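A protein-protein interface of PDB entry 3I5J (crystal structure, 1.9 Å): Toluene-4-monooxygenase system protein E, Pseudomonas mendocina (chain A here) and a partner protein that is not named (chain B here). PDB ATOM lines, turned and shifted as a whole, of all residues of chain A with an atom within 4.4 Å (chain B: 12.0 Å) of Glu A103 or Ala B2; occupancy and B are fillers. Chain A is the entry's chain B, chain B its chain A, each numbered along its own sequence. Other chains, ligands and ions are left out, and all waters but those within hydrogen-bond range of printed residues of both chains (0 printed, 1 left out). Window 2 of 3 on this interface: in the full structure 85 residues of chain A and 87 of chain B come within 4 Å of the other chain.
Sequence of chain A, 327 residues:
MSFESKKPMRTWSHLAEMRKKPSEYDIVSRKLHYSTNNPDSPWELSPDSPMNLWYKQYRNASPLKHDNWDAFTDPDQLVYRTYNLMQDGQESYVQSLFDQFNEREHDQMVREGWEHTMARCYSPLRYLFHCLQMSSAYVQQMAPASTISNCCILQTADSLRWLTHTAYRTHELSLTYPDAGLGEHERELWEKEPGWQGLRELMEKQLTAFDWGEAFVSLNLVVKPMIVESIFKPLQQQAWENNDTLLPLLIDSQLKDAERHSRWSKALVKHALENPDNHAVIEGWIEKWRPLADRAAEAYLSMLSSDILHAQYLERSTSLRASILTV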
ATOM      1  N   PHE A  98       8.974  -0.074 -24.976  1.00  0.00           N
ATOM      2  CA  PHE A  98      10.425  -0.120 -25.141  1.00  0.00           C
ATOM      3  C   PHE A  98      10.993  -1.474 -24.629  1.00  0.00           C
ATOM      4  O   PHE A  98      11.792  -2.111 -25.302  1.00  0.00           O
ATOM      5  CB  PHE A  98      11.143   1.007 -24.412  1.00  0.00           C
ATOM      6  CG  PHE A  98      10.906   2.389 -24.979  1.00  0.00           C
ATOM      7  CD1 PHE A  98      11.239   3.505 -24.226  1.00  0.00           C
ATOM      8  CD2 PHE A  98      10.346   2.575 -26.239  1.00  0.00           C
ATOM      9  CE1 PHE A  98      11.076   4.856 -24.733  1.00  0.00           C
ATOM     10  CE2 PHE A  98      10.161   3.948 -26.763  1.00  0.00           C
ATOM     11  CZ  PHE A  98      10.522   5.057 -26.007  1.00  0.00           C
ATOM     12  N   ASP A  99      10.588  -1.882 -23.419  1.00  0.00           N
ATOM     13  CA  ASP A  99      11.086  -3.110 -22.827  1.00  0.00           C
ATOM     14  C   ASP A  99      10.761  -4.302 -23.713  1.00  0.00           C
ATOM     15  O   ASP A  99      11.629  -5.090 -23.958  1.00  0.00           O
ATOM     16  CB  ASP A  99      10.486  -3.276 -21.428  1.00  0.00           C
ATOM     17  CG  ASP A  99      11.057  -4.478 -20.683  1.00  0.00           C
ATOM     18  OD1 ASP A  99      12.115  -4.956 -21.042  1.00  0.00           O
ATOM     19  OD2 ASP A  99      10.466  -4.880 -19.696  1.00  0.00           O
ATOM     20  N   GLN A 100       9.495  -4.453 -24.167  1.00  0.00           N
ATOM     21  CA  GLN A 100       9.037  -5.600 -24.911  1.00  0.00           C
ATOM     22  C   GLN A 100       9.670  -5.658 -26.338  1.00  0.00           C
ATOM     23  O   GLN A 100      10.089  -6.754 -26.815  1.00  0.00           O
ATOM     24  CB  GLN A 100       7.489  -5.604 -24.962  1.00  0.00           C
ATOM     25  CG  GLN A 100       6.959  -6.803 -25.738  1.00  0.00           C
ATOM     26  CD  GLN A 100       7.558  -8.121 -25.209  1.00  0.00           C
ATOM     27  OE1 GLN A 100       7.758  -8.296 -23.987  1.00  0.00           O
ATOM     28  NE2 GLN A 100       7.891  -9.031 -26.128  1.00  0.00           N
ATOM     29  N   PHE A 101       9.771  -4.489 -26.995  1.00  0.00           N
ATOM     30  CA  PHE A 101      10.280  -4.426 -28.336  1.00  0.00           C
ATOM     31  C   PHE A 101      11.806  -4.648 -28.319  1.00  0.00           C
ATOM     32  O   PHE A 101      12.385  -5.334 -29.178  1.00  0.00           O
ATOM     33  CB  PHE A 101       9.882  -3.088 -28.957  1.00  0.00           C
ATOM     34  CG  PHE A 101       8.517  -3.086 -29.569  1.00  0.00           C
ATOM     35  CD1 PHE A 101       8.365  -3.001 -30.969  1.00  0.00           C
ATOM     36  CD2 PHE A 101       7.400  -3.200 -28.799  1.00  0.00           C
ATOM     37  CE1 PHE A 101       7.069  -2.978 -31.543  1.00  0.00           C
ATOM     38  CE2 PHE A 101       6.086  -3.211 -29.381  1.00  0.00           C
ATOM     39  CZ  PHE A 101       5.948  -3.096 -30.764  1.00  0.00           C
ATOM     40  N   ASN A 102      12.447  -4.176 -27.265  1.00  0.00           N
ATOM     41  CA  ASN A 102      13.836  -4.567 -27.007  1.00  0.00           C
ATOM     42  C   ASN A 102      14.020  -6.084 -26.805  1.00  0.00           C
ATOM     43  O   ASN A 102      14.902  -6.739 -27.441  1.00  0.00           O
ATOM     44  CB  ASN A 102      14.401  -3.793 -25.796  1.00  0.00           C
ATOM     45  CG  ASN A 102      15.807  -4.267 -25.417  1.00  0.00           C
ATOM     46  OD1 ASN A 102      16.797  -3.730 -25.896  1.00  0.00           O
ATOM     47  ND2 ASN A 102      15.894  -5.219 -24.531  1.00  0.00           N
ATOM     48  N   GLU A 103      13.163  -6.691 -25.993  1.00  0.00           N
ATOM     49  CA  GLU A 103      13.248  -8.142 -25.824  1.00  0.00           C
ATOM     50  C   GLU A 103      13.170  -8.870 -27.154  1.00  0.00           C
ATOM     51  O   GLU A 103      13.841  -9.924 -27.389  1.00  0.00           O
ATOM     52  CB  GLU A 103      12.122  -8.684 -24.937  1.00  0.00           C
ATOM     53  CG  GLU A 103      12.209  -8.288 -23.484  1.00  0.00           C
ATOM     54  CD  GLU A 103      13.411  -8.913 -22.811  1.00  0.00           C
ATOM     55  OE1 GLU A 103      14.322  -8.146 -22.346  1.00  0.00           O
ATOM     56  OE2 GLU A 103      13.443 -10.183 -22.763  1.00  0.00           O
ATOM     57  N   ARG A 104      12.310  -8.363 -28.009  1.00  0.00           N
ATOM     58  CA  ARG A 104      12.077  -8.989 -29.290  1.00  0.00           C
ATOM     59  C   ARG A 104      13.145  -8.613 -30.330  1.00  0.00           C
ATOM     60  O   ARG A 104      13.085  -9.084 -31.489  1.00  0.00           O
ATOM     61  CB  ARG A 104      10.685  -8.598 -29.785  1.00  0.00           C
ATOM     62  CG  ARG A 104       9.573  -9.490 -29.226  1.00  0.00           C
ATOM     63  CD  ARG A 104       8.292  -8.687 -28.901  1.00  0.00           C
ATOM     64  NE  ARG A 104       7.574  -8.204 -30.096  1.00  0.00           N
ATOM     65  CZ  ARG A 104       6.324  -8.541 -30.426  1.00  0.00           C
ATOM     66  NH1 ARG A 104       5.784  -8.049 -31.524  1.00  0.00           N
ATOM     67  NH2 ARG A 104       5.597  -9.363 -29.667  1.00  0.00           N
ATOM     68  N   GLU A 105      14.132  -7.821 -29.918  1.00  0.00           N
ATOM     69  CA  GLU A 105      15.200  -7.407 -30.814  1.00  0.00           C
ATOM     70  C   GLU A 105      14.583  -6.749 -32.041  1.00  0.00           C
ATOM     71  O   GLU A 105      14.990  -7.031 -33.149  1.00  0.00           O
ATOM     72  CB  GLU A 105      16.126  -8.587 -31.223  1.00  0.00           C
ATOM     73  CG  GLU A 105      16.868  -9.278 -30.067  1.00  0.00           C
ATOM     74  CD  GLU A 105      17.518 -10.647 -30.464  1.00  0.00           C
ATOM     75  OE1 GLU A 105      16.812 -11.672 -30.711  1.00  0.00           O
ATOM     76  OE2 GLU A 105      18.776 -10.718 -30.524  1.00  0.00           O
ATOM     77  N   TYR A 168      16.441   8.472 -25.294  1.00  0.00           N
ATOM     78  CA  TYR A 168      16.442   7.039 -24.935  1.00  0.00           C
ATOM     79  C   TYR A 168      16.593   6.177 -26.177  1.00  0.00           C
ATOM     80  O   TYR A 168      17.431   5.242 -26.241  1.00  0.00           O
ATOM     81  CB  TYR A 168      15.150   6.659 -24.166  1.00  0.00           C
ATOM     82  CG  TYR A 168      15.167   5.200 -23.685  1.00  0.00           C
ATOM     83  CD1 TYR A 168      15.659   4.883 -22.430  1.00  0.00           C
ATOM     84  CD2 TYR A 168      14.749   4.152 -24.527  1.00  0.00           C
ATOM     85  CE1 TYR A 168      15.671   3.550 -21.962  1.00  0.00           C
ATOM     86  CE2 TYR A 168      14.824   2.766 -24.093  1.00  0.00           C
ATOM     87  CZ  TYR A 168      15.280   2.511 -22.814  1.00  0.00           C
ATOM     88  OH  TYR A 168      15.372   1.204 -22.341  1.00  0.00           O
ATOM     89  N   ALA B   2      14.389  -5.673 -22.219  1.00  0.00           N
ATOM     90  CA  ALA B   2      15.267  -5.003 -21.237  1.00  0.00           C
ATOM     91  C   ALA B   2      15.134  -3.484 -21.366  1.00  0.00           C
ATOM     92  O   ALA B   2      14.767  -3.002 -22.425  1.00  0.00           O
ATOM     93  CB  ALA B   2      16.729  -5.443 -21.421  1.00  0.00           C
ATOM     94  N   MET B   3      15.385  -2.754 -20.270  1.00  0.00           N
ATOM     95  CA  MET B   3      15.479  -1.289 -20.214  1.00  0.00           C
ATOM     96  C   MET B   3      16.951  -0.972 -20.033  1.00  0.00           C
ATOM     97  O   MET B   3      17.731  -1.836 -19.582  1.00  0.00           O
ATOM     98  CB  MET B   3      14.661  -0.713 -19.098  1.00  0.00           C
ATOM     99  CG  MET B   3      13.206  -1.170 -19.149  1.00  0.00           C
ATOM    100  SD  MET B   3      12.486  -0.534 -20.708  1.00  0.00           S
ATOM    101  CE  MET B   3      12.503   1.252 -20.272  1.00  0.00           C
ATOM    102  N   HIS B   4      17.388   0.152 -20.542  1.00  0.00           N
ATOM    103  CA  HIS B   4      18.768   0.593 -20.360  1.00  0.00           C
ATOM    104  C   HIS B   4      18.876   1.569 -19.191  1.00  0.00           C
ATOM    105  O   HIS B   4      17.990   2.330 -18.977  1.00  0.00           O
ATOM    106  CB  HIS B   4      19.238   1.215 -21.657  1.00  0.00           C
ATOM    107  CG  HIS B   4      19.043   0.303 -22.817  1.00  0.00           C
ATOM    108  ND1 HIS B   4      19.681  -0.919 -22.908  1.00  0.00           N
ATOM    109  CD2 HIS B   4      18.217   0.381 -23.891  1.00  0.00           C
ATOM    110  CE1 HIS B   4      19.280  -1.539 -24.012  1.00  0.00           C
ATOM    111  NE2 HIS B   4      18.415  -0.758 -24.646  1.00  0.00           N
ATOM    112  N   PRO B   5      19.957   1.481 -18.397  1.00  0.00           N
ATOM    113  CA  PRO B   5      20.005   2.303 -17.199  1.00  0.00           C
ATOM    114  C   PRO B   5      20.208   3.801 -17.512  1.00  0.00           C
ATOM    115  O   PRO B   5      20.790   4.166 -18.536  1.00  0.00           O
ATOM    116  CB  PRO B   5      21.227   1.757 -16.427  1.00  0.00           C
ATOM    117  CG  PRO B   5      22.028   1.000 -17.407  1.00  0.00           C
ATOM    118  CD  PRO B   5      21.045   0.485 -18.436  1.00  0.00           C
ATOM    119  N   ARG B   6      19.716   4.625 -16.625  1.00  0.00           N
ATOM    120  CA  ARG B   6      19.662   6.086 -16.889  1.00  0.00           C
ATOM    121  C   ARG B   6      21.066   6.595 -17.163  1.00  0.00           C
ATOM    122  O   ARG B   6      21.267   7.451 -18.031  1.00  0.00           O
ATOM    123  CB  ARG B   6      19.030   6.800 -15.712  1.00  0.00           C
ATOM    124  CG  ARG B   6      18.922   8.365 -15.962  1.00  0.00           C
ATOM    125  CD  ARG B   6      18.235   8.990 -14.723  1.00  0.00           C
ATOM    126  NE  ARG B   6      19.214   9.143 -13.629  1.00  0.00           N
ATOM    127  CZ  ARG B   6      18.888   9.383 -12.365  1.00  0.00           C
ATOM    128  NH1 ARG B   6      17.597   9.503 -12.009  1.00  0.00           N
ATOM    129  NH2 ARG B   6      19.857   9.549 -11.464  1.00  0.00           N
ATOM    130  N   ASP B   8      23.341   5.547 -18.901  1.00  0.00           N
ATOM    131  CA  ASP B   8      23.776   5.278 -20.271  1.00  0.00           C
ATOM    132  C   ASP B   8      23.208   6.241 -21.307  1.00  0.00           C
ATOM    133  O   ASP B   8      23.765   6.367 -22.384  1.00  0.00           O
ATOM    134  CB  ASP B   8      23.363   3.866 -20.694  1.00  0.00           C
ATOM    135  CG  ASP B   8      24.184   2.769 -19.987  1.00  0.00           C
ATOM    136  OD1 ASP B   8      25.052   3.126 -19.178  1.00  0.00           O
ATOM    137  OD2 ASP B   8      23.916   1.576 -20.228  1.00  0.00           O
ATOM    138  N   TRP B   9      22.086   6.879 -21.000  1.00  0.00           N
ATOM    139  CA  TRP B   9      21.407   7.752 -21.951  1.00  0.00           C
ATOM    140  C   TRP B   9      21.167   9.151 -21.343  1.00  0.00           C
ATOM    141  O   TRP B   9      20.699  10.052 -22.025  1.00  0.00           O
ATOM    142  CB  TRP B   9      20.059   7.112 -22.469  1.00  0.00           C
ATOM    143  CG  TRP B   9      19.118   6.590 -21.344  1.00  0.00           C
ATOM    144  CD1 TRP B   9      19.015   5.305 -20.906  1.00  0.00           C
ATOM    145  CD2 TRP B   9      18.181   7.360 -20.528  1.00  0.00           C
ATOM    146  NE1 TRP B   9      18.094   5.208 -19.880  1.00  0.00           N
ATOM    147  CE2 TRP B   9      17.562   6.453 -19.639  1.00  0.00           C
ATOM    148  CE3 TRP B   9      17.835   8.724 -20.469  1.00  0.00           C
ATOM    149  CZ2 TRP B   9      16.646   6.863 -18.639  1.00  0.00           C
ATOM    150  CZ3 TRP B   9      16.886   9.158 -19.462  1.00  0.00           C
ATOM    151  CH2 TRP B   9      16.283   8.217 -18.620  1.00  0.00           C
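The backbone NH (N) of Ala B2 is in hydrogen-bond range of the side-chain carboxylate (OD1) of Asp A99 (2.7 Å).
N of Ala B2 lies close to ND2 of Asn A102 (2.8 Å).
The backbone NH of Ala B2 sits at hydrogen-bond distance from the side-chain carboxylate of Glu A103.
The side-chain sulfur of Met B3 sits close to the backbone NH of Asp A99 (3.6 Å).
SD of Met B3 sits close to OH of Tyr A168, at 3.7 Å.
N of His B4 sits at hydrogen-bond distance from OH of Tyr A168, at 2.9 Å.
O of His B4 sits at hydrogen-bond distance from NE1 of Trp B9 (3.0 Å).
NE1 of Trp B9 lies close to O of Pro B5 (3.2 Å).
NE2 of His B4 touches OD1 of Asn A102, 3.6 Å away.
Trp B9 touches Tyr A168 (NE1 to CD1, 3.5 Å).
No residue of chain B comes within 4 Å of Gln A100.
Of chain B, only Ala B2 (2.8 Å) and His B4 (3.6 Å) come within 4 Å of Asn A102.
Glu A103 touches just one residue of chain B: Ala B2.
Arg A104 touches none of the printed residues of chain B.
No residue of chain B comes within 4 Å of Glu A105.
Printed residues of chain B within 4 Å of Tyr A168: Met B3 (3.3 Å), His B4 (2.9 Å) and Trp B9 (3.5 Å).
Of the printed residues of chain A, Met B3 touches Asp A99 (3.5 Å) and Tyr A168 (3.3 Å).
Of the printed residues of chain A, His B4 touches Asn A102 and Tyr A168.
Pro B5 touches none of the printed residues of chain A.
Of the printed residues of chain A, Trp B9 touches Tyr A168 (3.5 Å).
The nearest printed residue of chain A that does not touch Ala B2 is Phe A98 (4.2 Å).
The nearest printed residue of chain A that does not touch Trp B9 is Phe A98 (8.3 Å).
Hydrophobic or aromatic side chains of chain A that line the printed part of chain B: Tyr A168.
Hydrophobic or aromatic side chains of chain B that line the printed part of chain A: Ala B2, Met B3, His B4 and Trp B9.
Among the printed residues, 8 pairs touch across the chains.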
